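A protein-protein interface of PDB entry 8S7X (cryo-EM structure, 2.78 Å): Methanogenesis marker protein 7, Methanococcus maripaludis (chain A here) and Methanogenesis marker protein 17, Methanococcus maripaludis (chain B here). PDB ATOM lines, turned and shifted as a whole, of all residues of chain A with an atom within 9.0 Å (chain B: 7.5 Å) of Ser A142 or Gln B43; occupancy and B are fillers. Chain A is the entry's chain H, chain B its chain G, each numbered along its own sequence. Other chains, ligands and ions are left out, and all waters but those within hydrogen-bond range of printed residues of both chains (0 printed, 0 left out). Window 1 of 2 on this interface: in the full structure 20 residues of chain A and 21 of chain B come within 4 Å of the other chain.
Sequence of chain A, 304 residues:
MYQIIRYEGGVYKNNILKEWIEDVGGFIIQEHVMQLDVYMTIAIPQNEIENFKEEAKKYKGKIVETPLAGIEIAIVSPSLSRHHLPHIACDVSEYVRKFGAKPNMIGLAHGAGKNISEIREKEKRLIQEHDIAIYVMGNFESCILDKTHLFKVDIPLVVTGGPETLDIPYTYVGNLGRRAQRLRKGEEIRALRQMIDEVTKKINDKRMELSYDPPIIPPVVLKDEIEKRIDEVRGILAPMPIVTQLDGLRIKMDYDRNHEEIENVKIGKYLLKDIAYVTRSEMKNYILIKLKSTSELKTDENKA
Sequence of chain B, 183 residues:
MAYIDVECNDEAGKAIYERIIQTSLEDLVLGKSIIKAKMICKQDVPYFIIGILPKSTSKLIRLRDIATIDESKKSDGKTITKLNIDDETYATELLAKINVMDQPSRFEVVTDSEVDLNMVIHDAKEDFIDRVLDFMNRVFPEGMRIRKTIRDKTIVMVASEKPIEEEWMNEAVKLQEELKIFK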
ATOM      1  N   GLY A 113      -6.675  -1.197  28.451  1.00  0.00           N
ATOM      2  CA  GLY A 113      -6.926  -0.069  27.576  1.00  0.00           C
ATOM      3  C   GLY A 113      -6.987   1.236  28.342  1.00  0.00           C
ATOM      4  O   GLY A 113      -6.876   1.288  29.572  1.00  0.00           O
ATOM      5  N   LYS A 114      -7.163   2.318  27.585  1.00  0.00           N
ATOM      6  CA  LYS A 114      -7.264   3.657  28.156  1.00  0.00           C
ATOM      7  C   LYS A 114      -8.708   4.133  28.243  1.00  0.00           C
ATOM      8  O   LYS A 114      -9.196   4.454  29.328  1.00  0.00           O
ATOM      9  CB  LYS A 114      -6.427   4.644  27.334  1.00  0.00           C
ATOM     10  CG  LYS A 114      -6.190   5.967  28.034  1.00  0.00           C
ATOM     11  CD  LYS A 114      -5.304   6.879  27.212  1.00  0.00           C
ATOM     12  CE  LYS A 114      -5.474   8.324  27.631  1.00  0.00           C
ATOM     13  NZ  LYS A 114      -4.184   9.055  27.615  1.00  0.00           N
ATOM     14  N   ASN A 115      -9.406   4.186  27.112  1.00  0.00           N
ATOM     15  CA  ASN A 115     -10.799   4.603  27.076  1.00  0.00           C
ATOM     16  C   ASN A 115     -11.753   3.444  26.838  1.00  0.00           C
ATOM     17  O   ASN A 115     -12.969   3.656  26.818  1.00  0.00           O
ATOM     18  CB  ASN A 115     -11.008   5.667  25.993  1.00  0.00           C
ATOM     19  CG  ASN A 115      -9.800   6.557  25.813  1.00  0.00           C
ATOM     20  OD1 ASN A 115      -9.235   7.059  26.782  1.00  0.00           O
ATOM     21  ND2 ASN A 115      -9.395   6.755  24.564  1.00  0.00           N
ATOM     22  N   GLY A 138      -1.177   0.515  35.674  1.00  0.00           N
ATOM     23  CA  GLY A 138      -0.046   0.660  34.783  1.00  0.00           C
ATOM     24  C   GLY A 138       0.943   1.705  35.242  1.00  0.00           C
ATOM     25  O   GLY A 138       0.993   2.078  36.415  1.00  0.00           O
ATOM     26  N   ASN A 139       1.747   2.186  34.296  1.00  0.00           N
ATOM     27  CA  ASN A 139       2.828   3.106  34.627  1.00  0.00           C
ATOM     28  C   ASN A 139       2.787   4.370  33.777  1.00  0.00           C
ATOM     29  O   ASN A 139       3.831   4.906  33.406  1.00  0.00           O
ATOM     30  CB  ASN A 139       4.191   2.427  34.501  1.00  0.00           C
ATOM     31  CG  ASN A 139       4.242   1.432  33.372  1.00  0.00           C
ATOM     32  OD1 ASN A 139       3.913   1.752  32.236  1.00  0.00           O
ATOM     33  ND2 ASN A 139       4.662   0.216  33.676  1.00  0.00           N
ATOM     34  N   PHE A 140       1.595   4.867  33.465  1.00  0.00           N
ATOM     35  CA  PHE A 140       1.438   6.139  32.776  1.00  0.00           C
ATOM     36  C   PHE A 140       0.412   6.976  33.519  1.00  0.00           C
ATOM     37  O   PHE A 140      -0.703   6.513  33.775  1.00  0.00           O
ATOM     38  CB  PHE A 140       1.016   5.943  31.318  1.00  0.00           C
ATOM     39  CG  PHE A 140       2.078   5.324  30.462  1.00  0.00           C
ATOM     40  CD1 PHE A 140       3.373   5.799  30.491  1.00  0.00           C
ATOM     41  CD2 PHE A 140       1.782   4.264  29.628  1.00  0.00           C
ATOM     42  CE1 PHE A 140       4.350   5.227  29.709  1.00  0.00           C
ATOM     43  CE2 PHE A 140       2.754   3.691  28.843  1.00  0.00           C
ATOM     44  CZ  PHE A 140       4.036   4.173  28.881  1.00  0.00           C
ATOM     45  N   GLU A 141       0.788   8.212  33.851  1.00  0.00           N
ATOM     46  CA  GLU A 141      -0.077   9.060  34.661  1.00  0.00           C
ATOM     47  C   GLU A 141      -1.388   9.359  33.954  1.00  0.00           C
ATOM     48  O   GLU A 141      -2.458   9.320  34.571  1.00  0.00           O
ATOM     49  CB  GLU A 141       0.648  10.357  35.008  1.00  0.00           C
ATOM     50  CG  GLU A 141       0.297  10.916  36.368  1.00  0.00           C
ATOM     51  CD  GLU A 141       1.475  11.572  37.050  1.00  0.00           C
ATOM     52  OE1 GLU A 141       2.482  10.879  37.295  1.00  0.00           O
ATOM     53  OE2 GLU A 141       1.395  12.784  37.342  1.00  0.00           O
ATOM     54  N   SER A 142      -1.331   9.667  32.655  1.00  0.00           N
ATOM     55  CA  SER A 142      -2.549   9.980  31.917  1.00  0.00           C
ATOM     56  C   SER A 142      -3.487   8.783  31.854  1.00  0.00           C
ATOM     57  O   SER A 142      -4.704   8.928  32.036  1.00  0.00           O
ATOM     58  CB  SER A 142      -2.200  10.453  30.508  1.00  0.00           C
ATOM     59  OG  SER A 142      -3.185  10.033  29.584  1.00  0.00           O
ATOM     60  N   CYS A 143      -2.941   7.595  31.591  1.00  0.00           N
ATOM     61  CA  CYS A 143      -3.773   6.402  31.492  1.00  0.00           C
ATOM     62  C   CYS A 143      -4.468   6.107  32.813  1.00  0.00           C
ATOM     63  O   CYS A 143      -5.658   5.774  32.835  1.00  0.00           O
ATOM     64  CB  CYS A 143      -2.926   5.208  31.052  1.00  0.00           C
ATOM     65  SG  CYS A 143      -2.551   5.166  29.288  1.00  0.00           S
ATOM     66  N   ILE A 144      -3.744   6.227  33.927  1.00  0.00           N
ATOM     67  CA  ILE A 144      -4.351   5.992  35.231  1.00  0.00           C
ATOM     68  C   ILE A 144      -5.402   7.051  35.531  1.00  0.00           C
ATOM     69  O   ILE A 144      -6.491   6.738  36.026  1.00  0.00           O
ATOM     70  CB  ILE A 144      -3.269   5.942  36.325  1.00  0.00           C
ATOM     71  CG1 ILE A 144      -2.360   4.730  36.123  1.00  0.00           C
ATOM     72  CG2 ILE A 144      -3.898   5.910  37.704  1.00  0.00           C
ATOM     73  CD1 ILE A 144      -1.216   4.665  37.100  1.00  0.00           C
ATOM     74  N   LEU A 145      -5.100   8.314  35.238  1.00  0.00           N
ATOM     75  CA  LEU A 145      -6.045   9.383  35.541  1.00  0.00           C
ATOM     76  C   LEU A 145      -7.326   9.241  34.737  1.00  0.00           C
ATOM     77  O   LEU A 145      -8.402   9.616  35.213  1.00  0.00           O
ATOM     78  CB  LEU A 145      -5.401  10.742  35.276  1.00  0.00           C
ATOM     79  CG  LEU A 145      -4.525  11.289  36.401  1.00  0.00           C
ATOM     80  CD1 LEU A 145      -4.103  12.714  36.094  1.00  0.00           C
ATOM     81  CD2 LEU A 145      -5.283  11.226  37.713  1.00  0.00           C
ATOM     82  N   ASP A 146      -7.230   8.695  33.523  1.00  0.00           N
ATOM     83  CA  ASP A 146      -8.393   8.485  32.671  1.00  0.00           C
ATOM     84  C   ASP A 146      -8.941   7.067  32.913  1.00  0.00           C
ATOM     85  O   ASP A 146      -9.363   6.360  31.999  1.00  0.00           O
ATOM     86  CB  ASP A 146      -7.966   8.786  31.216  1.00  0.00           C
ATOM     87  CG  ASP A 146      -8.991   8.409  30.113  1.00  0.00           C
ATOM     88  OD1 ASP A 146     -10.021   7.750  30.327  1.00  0.00           O
ATOM     89  OD2 ASP A 146      -8.727   8.814  28.953  1.00  0.00           O
ATOM     90  N   LYS A 147      -8.824   6.584  34.152  1.00  0.00           N
ATOM     91  CA  LYS A 147      -9.250   5.231  34.486  1.00  0.00           C
ATOM     92  C   LYS A 147      -9.868   5.167  35.877  1.00  0.00           C
ATOM     93  O   LYS A 147      -9.982   4.074  36.443  1.00  0.00           O
ATOM     94  CB  LYS A 147      -8.071   4.253  34.403  1.00  0.00           C
ATOM     95  CG  LYS A 147      -8.355   2.959  33.657  1.00  0.00           C
ATOM     96  CD  LYS A 147      -7.111   2.086  33.570  1.00  0.00           C
ATOM     97  CE  LYS A 147      -7.347   0.914  32.647  1.00  0.00           C
ATOM     98  NZ  LYS A 147      -6.076   0.299  32.211  1.00  0.00           N
ATOM     99  N   THR A 148     -10.252   6.314  36.445  1.00  0.00           N
ATOM    100  CA  THR A 148     -10.751   6.355  37.816  1.00  0.00           C
ATOM    101  C   THR A 148     -12.065   5.596  37.963  1.00  0.00           C
ATOM    102  O   THR A 148     -12.352   5.062  39.043  1.00  0.00           O
ATOM    103  CB  THR A 148     -10.888   7.817  38.264  1.00  0.00           C
ATOM    104  OG1 THR A 148      -9.609   8.305  38.685  1.00  0.00           O
ATOM    105  CG2 THR A 148     -11.880   7.978  39.405  1.00  0.00           C
ATOM    106  N   PRO A 163       3.912   5.627  38.189  1.00  0.00           N
ATOM    107  CA  PRO A 163       4.353   6.945  38.658  1.00  0.00           C
ATOM    108  C   PRO A 163       4.434   7.010  40.172  1.00  0.00           C
ATOM    109  O   PRO A 163       3.651   6.385  40.886  1.00  0.00           O
ATOM    110  CB  PRO A 163       3.272   7.886  38.118  1.00  0.00           C
ATOM    111  CG  PRO A 163       2.758   7.200  36.921  1.00  0.00           C
ATOM    112  CD  PRO A 163       2.791   5.740  37.241  1.00  0.00           C
ATOM    113  N   THR A 165       3.845   9.484  42.216  1.00  0.00           N
ATOM    114  CA  THR A 165       2.757  10.200  42.868  1.00  0.00           C
ATOM    115  C   THR A 165       1.630  10.419  41.872  1.00  0.00           C
ATOM    116  O   THR A 165       1.877  10.832  40.736  1.00  0.00           O
ATOM    117  CB  THR A 165       3.242  11.542  43.425  1.00  0.00           C
ATOM    118  OG1 THR A 165       3.947  11.326  44.654  1.00  0.00           O
ATOM    119  CG2 THR A 165       2.071  12.477  43.680  1.00  0.00           C
ATOM    120  N   LEU A 166       0.401  10.142  42.298  1.00  0.00           N
ATOM    121  CA  LEU A 166      -0.777  10.333  41.471  1.00  0.00           C
ATOM    122  C   LEU A 166      -1.725  11.321  42.135  1.00  0.00           C
ATOM    123  O   LEU A 166      -1.627  11.605  43.331  1.00  0.00           O
ATOM    124  CB  LEU A 166      -1.500   9.009  41.217  1.00  0.00           C
ATOM    125  CG  LEU A 166      -1.502   8.521  39.774  1.00  0.00           C
ATOM    126  CD1 LEU A 166      -2.496   9.311  38.954  1.00  0.00           C
ATOM    127  CD2 LEU A 166      -0.116   8.643  39.189  1.00  0.00           C
ATOM    128  N   ILE A 168      -5.231  11.037  42.104  1.00  0.00           N
ATOM    129  CA  ILE A 168      -6.552  10.421  42.161  1.00  0.00           C
ATOM    130  C   ILE A 168      -7.118  10.621  43.562  1.00  0.00           C
ATOM    131  O   ILE A 168      -6.348  10.733  44.526  1.00  0.00           O
ATOM    132  CB  ILE A 168      -6.487   8.931  41.795  1.00  0.00           C
ATOM    133  CG1 ILE A 168      -5.349   8.252  42.559  1.00  0.00           C
ATOM    134  CG2 ILE A 168      -6.306   8.762  40.302  1.00  0.00           C
ATOM    135  CD1 ILE A 168      -5.328   6.751  42.414  1.00  0.00           C
ATOM    136  N   GLU B   7      11.139   7.253  24.118  1.00  0.00           N
ATOM    137  CA  GLU B   7      10.748   8.650  23.965  1.00  0.00           C
ATOM    138  C   GLU B   7       9.389   8.836  24.629  1.00  0.00           C
ATOM    139  O   GLU B   7       8.348   8.573  24.024  1.00  0.00           O
ATOM    140  CB  GLU B   7      10.709   9.037  22.490  1.00  0.00           C
ATOM    141  CG  GLU B   7      10.989  10.505  22.227  1.00  0.00           C
ATOM    142  CD  GLU B   7      10.474  10.961  20.876  1.00  0.00           C
ATOM    143  OE1 GLU B   7      11.070  10.579  19.848  1.00  0.00           O
ATOM    144  OE2 GLU B   7       9.471  11.707  20.843  1.00  0.00           O
ATOM    145  N   CYS B   8       9.401   9.293  25.879  1.00  0.00           N
ATOM    146  CA  CYS B   8       8.176   9.514  26.628  1.00  0.00           C
ATOM    147  C   CYS B   8       8.353  10.712  27.544  1.00  0.00           C
ATOM    148  O   CYS B   8       9.438  10.944  28.087  1.00  0.00           O
ATOM    149  CB  CYS B   8       7.783   8.286  27.454  1.00  0.00           C
ATOM    150  SG  CYS B   8       6.075   8.302  28.032  1.00  0.00           S
ATOM    151  N   ASN B   9       7.274  11.470  27.716  1.00  0.00           N
ATOM    152  CA  ASN B   9       7.264  12.604  28.627  1.00  0.00           C
ATOM    153  C   ASN B   9       6.933  12.209  30.060  1.00  0.00           C
ATOM    154  O   ASN B   9       6.949  13.070  30.944  1.00  0.00           O
ATOM    155  CB  ASN B   9       6.288  13.676  28.113  1.00  0.00           C
ATOM    156  CG  ASN B   9       4.829  13.256  28.206  1.00  0.00           C
ATOM    157  OD1 ASN B   9       4.360  12.766  29.232  1.00  0.00           O
ATOM    158  ND2 ASN B   9       4.099  13.453  27.116  1.00  0.00           N
ATOM    159  N   ASP B  10       6.637  10.936  30.305  1.00  0.00           N
ATOM    160  CA  ASP B  10       6.395  10.416  31.643  1.00  0.00           C
ATOM    161  C   ASP B  10       7.699   9.846  32.181  1.00  0.00           C
ATOM    162  O   ASP B  10       8.300   8.966  31.557  1.00  0.00           O
ATOM    163  CB  ASP B  10       5.306   9.345  31.621  1.00  0.00           C
ATOM    164  CG  ASP B  10       4.520   9.278  32.913  1.00  0.00           C
ATOM    165  OD1 ASP B  10       5.121   8.991  33.968  1.00  0.00           O
ATOM    166  OD2 ASP B  10       3.296   9.514  32.875  1.00  0.00           O
ATOM    167  N   GLU B  11       8.136  10.350  33.335  1.00  0.00           N
ATOM    168  CA  GLU B  11       9.424   9.936  33.876  1.00  0.00           C
ATOM    169  C   GLU B  11       9.408   8.468  34.279  1.00  0.00           C
ATOM    170  O   GLU B  11      10.302   7.702  33.900  1.00  0.00           O
ATOM    171  CB  GLU B  11       9.797  10.818  35.067  1.00  0.00           C
ATOM    172  CG  GLU B  11      11.281  10.829  35.402  1.00  0.00           C
ATOM    173  CD  GLU B  11      11.755   9.528  36.017  1.00  0.00           C
ATOM    174  OE1 GLU B  11      11.398   9.255  37.183  1.00  0.00           O
ATOM    175  OE2 GLU B  11      12.477   8.772  35.333  1.00  0.00           O
ATOM    176  N   GLY B  13       7.261   6.095  33.418  1.00  0.00           N
ATOM    177  CA  GLY B  13       7.007   5.241  32.272  1.00  0.00           C
ATOM    178  C   GLY B  13       8.259   4.970  31.465  1.00  0.00           C
ATOM    179  O   GLY B  13       8.477   3.849  31.005  1.00  0.00           O
ATOM    180  N   ILE B  40       8.582   4.693  21.067  1.00  0.00           N
ATOM    181  CA  ILE B  40       7.993   6.018  21.212  1.00  0.00           C
ATOM    182  C   ILE B  40       6.658   5.855  21.919  1.00  0.00           C
ATOM    183  O   ILE B  40       5.753   5.185  21.407  1.00  0.00           O
ATOM    184  CB  ILE B  40       7.813   6.713  19.854  1.00  0.00           C
ATOM    185  CG1 ILE B  40       9.170   7.016  19.228  1.00  0.00           C
ATOM    186  CG2 ILE B  40       7.002   7.983  20.016  1.00  0.00           C
ATOM    187  CD1 ILE B  40       9.225   6.733  17.753  1.00  0.00           C
ATOM    188  N   CYS B  41       6.532   6.469  23.089  1.00  0.00           N
ATOM    189  CA  CYS B  41       5.335   6.345  23.911  1.00  0.00           C
ATOM    190  C   CYS B  41       4.503   7.612  23.762  1.00  0.00           C
ATOM    191  O   CYS B  41       4.962   8.708  24.095  1.00  0.00           O
ATOM    192  CB  CYS B  41       5.701   6.105  25.371  1.00  0.00           C
ATOM    193  SG  CYS B  41       6.661   4.612  25.679  1.00  0.00           S
ATOM    194  N   LYS B  42       3.285   7.458  23.261  1.00  0.00           N
ATOM    195  CA  LYS B  42       2.295   8.530  23.220  1.00  0.00           C
ATOM    196  C   LYS B  42       1.063   8.009  23.946  1.00  0.00           C
ATOM    197  O   LYS B  42       0.278   7.243  23.380  1.00  0.00           O
ATOM    198  CB  LYS B  42       1.975   8.942  21.787  1.00  0.00           C
ATOM    199  CG  LYS B  42       3.189   9.369  20.987  1.00  0.00           C
ATOM    200  CD  LYS B  42       3.211  10.871  20.778  1.00  0.00           C
ATOM    201  CE  LYS B  42       4.636  11.396  20.763  1.00  0.00           C
ATOM    202  NZ  LYS B  42       5.134  11.681  22.136  1.00  0.00           N
ATOM    203  N   GLN B  43       0.902   8.407  25.205  1.00  0.00           N
ATOM    204  CA  GLN B  43      -0.206   7.924  26.015  1.00  0.00           C
ATOM    205  C   GLN B  43      -1.410   8.854  26.008  1.00  0.00           C
ATOM    206  O   GLN B  43      -2.534   8.386  26.205  1.00  0.00           O
ATOM    207  CB  GLN B  43       0.253   7.699  27.457  1.00  0.00           C
ATOM    208  CG  GLN B  43       0.782   8.938  28.139  1.00  0.00           C
ATOM    209  CD  GLN B  43       2.289   8.953  28.197  1.00  0.00           C
ATOM    210  OE1 GLN B  43       2.883   9.769  28.898  1.00  0.00           O
ATOM    211  NE2 GLN B  43       2.920   8.053  27.456  1.00  0.00           N
ATOM    212  N   ASP B  44      -1.205  10.155  25.788  1.00  0.00           N
ATOM    213  CA  ASP B  44      -2.336  11.077  25.739  1.00  0.00           C
ATOM    214  C   ASP B  44      -3.268  10.730  24.587  1.00  0.00           C
ATOM    215  O   ASP B  44      -4.490  10.680  24.751  1.00  0.00           O
ATOM    216  CB  ASP B  44      -1.830  12.511  25.631  1.00  0.00           C
ATOM    217  CG  ASP B  44      -0.847  12.861  26.732  1.00  0.00           C
ATOM    218  OD1 ASP B  44      -0.111  11.959  27.179  1.00  0.00           O
ATOM    219  OD2 ASP B  44      -0.813  14.035  27.154  1.00  0.00           O
ATOM    220  N   VAL B  45      -2.705  10.484  23.410  1.00  0.00           N
ATOM    221  CA  VAL B  45      -3.406   9.830  22.313  1.00  0.00           C
ATOM    222  C   VAL B  45      -2.877   8.401  22.247  1.00  0.00           C
ATOM    223  O   VAL B  45      -1.712   8.190  21.876  1.00  0.00           O
ATOM    224  CB  VAL B  45      -3.210  10.567  20.981  1.00  0.00           C
ATOM    225  CG1 VAL B  45      -1.802  11.137  20.879  1.00  0.00           C
ATOM    226  CG2 VAL B  45      -3.512   9.644  19.807  1.00  0.00           C
ATOM    227  N   PRO B  46      -3.670   7.400  22.595  1.00  0.00           N
ATOM    228  CA  PRO B  46      -3.091   6.078  22.862  1.00  0.00           C
ATOM    229  C   PRO B  46      -2.537   5.415  21.616  1.00  0.00           C
ATOM    230  O   PRO B  46      -3.291   4.911  20.781  1.00  0.00           O
ATOM    231  CB  PRO B  46      -4.274   5.284  23.433  1.00  0.00           C
ATOM    232  CG  PRO B  46      -5.308   6.303  23.786  1.00  0.00           C
ATOM    233  CD  PRO B  46      -5.117   7.433  22.842  1.00  0.00           C
ATOM    234  N   TYR B  47      -1.210   5.411  21.498  1.00  0.00           N
ATOM    235  CA  TYR B  47      -0.510   4.684  20.448  1.00  0.00           C
ATOM    236  C   TYR B  47       0.961   4.611  20.827  1.00  0.00           C
ATOM    237  O   TYR B  47       1.496   5.541  21.430  1.00  0.00           O
ATOM    238  CB  TYR B  47      -0.722   5.333  19.065  1.00  0.00           C
ATOM    239  CG  TYR B  47       0.136   6.533  18.689  1.00  0.00           C
ATOM    240  CD1 TYR B  47       1.506   6.415  18.482  1.00  0.00           C
ATOM    241  CD2 TYR B  47      -0.451   7.760  18.429  1.00  0.00           C
ATOM    242  CE1 TYR B  47       2.271   7.502  18.117  1.00  0.00           C
ATOM    243  CE2 TYR B  47       0.304   8.852  18.065  1.00  0.00           C
ATOM    244  CZ  TYR B  47       1.665   8.716  17.903  1.00  0.00           C
ATOM    245  OH  TYR B  47       2.419   9.801  17.531  1.00  0.00           O
ATOM    246  N   PHE B  48       1.594   3.493  20.492  1.00  0.00           N
ATOM    247  CA  PHE B  48       2.996   3.260  20.790  1.00  0.00           C
ATOM    248  C   PHE B  48       3.683   2.743  19.537  1.00  0.00           C
ATOM    249  O   PHE B  48       3.080   2.019  18.743  1.00  0.00           O
ATOM    250  CB  PHE B  48       3.173   2.252  21.932  1.00  0.00           C
ATOM    251  CG  PHE B  48       2.586   2.701  23.238  1.00  0.00           C
ATOM    252  CD1 PHE B  48       1.222   2.666  23.450  1.00  0.00           C
ATOM    253  CD2 PHE B  48       3.402   3.147  24.255  1.00  0.00           C
ATOM    254  CE1 PHE B  48       0.684   3.079  24.647  1.00  0.00           C
ATOM    255  CE2 PHE B  48       2.866   3.557  25.455  1.00  0.00           C
ATOM    256  CZ  PHE B  48       1.504   3.522  25.648  1.00  0.00           C
ATOM    257  N   MET B 144      -3.637  -1.974  23.625  1.00  0.00           N
ATOM    258  CA  MET B 144      -3.381  -1.607  22.235  1.00  0.00           C
ATOM    259  C   MET B 144      -3.385  -2.884  21.404  1.00  0.00           C
ATOM    260  O   MET B 144      -2.367  -3.559  21.252  1.00  0.00           O
ATOM    261  CB  MET B 144      -2.066  -0.855  22.111  1.00  0.00           C
ATOM    262  CG  MET B 144      -1.953   0.345  23.034  1.00  0.00           C
ATOM    263  SD  MET B 144      -3.557   0.990  23.532  1.00  0.00           S
ATOM    264  CE  MET B 144      -3.108   1.892  25.009  1.00  0.00           C
ATOM    265  N   GLU B 161      -5.445   1.304  20.476  1.00  0.00           N
ATOM    266  CA  GLU B 161      -6.790   0.792  20.696  1.00  0.00           C
ATOM    267  C   GLU B 161      -7.779   1.284  19.652  1.00  0.00           C
ATOM    268  O   GLU B 161      -8.888   0.747  19.568  1.00  0.00           O
ATOM    269  CB  GLU B 161      -7.280   1.179  22.092  1.00  0.00           C
ATOM    270  CG  GLU B 161      -7.823   2.591  22.180  1.00  0.00           C
ATOM    271  CD  GLU B 161      -7.536   3.239  23.518  1.00  0.00           C
ATOM    272  OE1 GLU B 161      -6.840   2.615  24.344  1.00  0.00           O
ATOM    273  OE2 GLU B 161      -8.010   4.375  23.741  1.00  0.00           O
ATOM    274  N   LYS B 162      -7.403   2.282  18.863  1.00  0.00           N
ATOM    275  CA  LYS B 162      -8.202   2.843  17.790  1.00  0.00           C
ATOM    276  C   LYS B 162      -7.623   2.440  16.440  1.00  0.00           C
ATOM    277  O   LYS B 162      -6.460   2.030  16.352  1.00  0.00           O
ATOM    278  CB  LYS B 162      -8.241   4.373  17.895  1.00  0.00           C
ATOM    279  CG  LYS B 162      -8.656   4.890  19.256  1.00  0.00           C
ATOM    280  CD  LYS B 162      -8.647   6.405  19.289  1.00  0.00           C
ATOM    281  CE  LYS B 162      -7.415   6.932  19.998  1.00  0.00           C
ATOM    282  NZ  LYS B 162      -7.744   8.075  20.892  1.00  0.00           N
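The backbone NH of Glu A141 sits at hydrogen-bond distance from the side-chain carboxylate of Asp B10.
NZ of Lys A114 is in hydrogen-bond range of O of Asp B44 (3.3 Å).
The side-chain carboxylate of Glu B161 sits at hydrogen-bond distance from the backbone NH of Lys A114 (3.3 Å).
The side-chain carboxylate (OE2) of Glu B161 lies within hydrogen-bond range of the side-chain amide nitrogen (ND2) of Asn A115, at 2.9 Å.
NZ of Lys A114 lies close to O of Gln B43 (2.3 Å).
The side-chain sulfur (SG) of Cys B8 sits close to the backbone NH (N) of Asp B10 (3.5 Å).
SG of Cys B8 sits at hydrogen-bond distance from NE2 of Gln B43 (3.2 Å).
The side-chain amide oxygen (OD1) of Asn B9 sits close to the side-chain amide oxygen (OE1) of Gln B43, at 3.4 Å.
SD of Met B144 sits at hydrogen-bond distance from N of Glu B161.
NZ of Lys A114 sits at hydrogen-bond distance from OG of Ser A142 (2.4 Å).
The side-chain carboxylate (OD2) of Asp A146 sits close to the side-chain amide oxygen (OD1) of Asn A115 (2.8 Å).
CD of Lys A114 touches CG of Pro B46 (3.5 Å).
Asn A139 touches Gly B13.
Cys B8 touches Phe A140.
CA of Phe A140 touches OD2 of Asp B10 (3.9 Å).
Gly B13 touches Phe A140 (CA to CE1, 3.7 Å).
Phe A140 touches Gln B43 (CD1 to NE2, 3.8 Å).
Phe B48 touches Phe A140 (CE2 to CE2, 3.4 Å).
Gln B43 touches Ser A142.
Of chain B, only Gln B43 comes within 4 Å of Ser A142.
Gln B43 touches three residues of chain A.
Of the printed residues of chain B, Asn A115 touches Glu B161 (2.9 Å).
Printed residues of chain A within 4 Å of Asp B10: Phe A140 and Glu A141.
Printed residues of chain A within 4 Å of Pro B46: Lys A114 (3.5 Å).
Printed residues of chain B within 4 Å of Lys A114: Gln B43 (2.3 Å), Asp B44 (3.3 Å), Pro B46 (3.5 Å) and Glu B161 (3.3 Å).
Glu B7 touches none of the printed residues of chain A.
The nearest residue of chain B that does not touch Ser A142 is Asp B44 (4.1 Å).
The nearest residue of chain A that does not touch Gln B43 is Cys A143 (4.2 Å).
Hydrophobic or aromatic side chains of chain A that line the printed part of chain B: Phe A140.
Of the 18 printed residues of chain B, 8 touch a printed residue of chain A.
Among the printed residues, 13 pairs touch across the chains.
Among the printed residues, no Asp or Glu carboxylate lies within 4 Å of a Lys or Arg side-chain nitrogen of the other chain.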
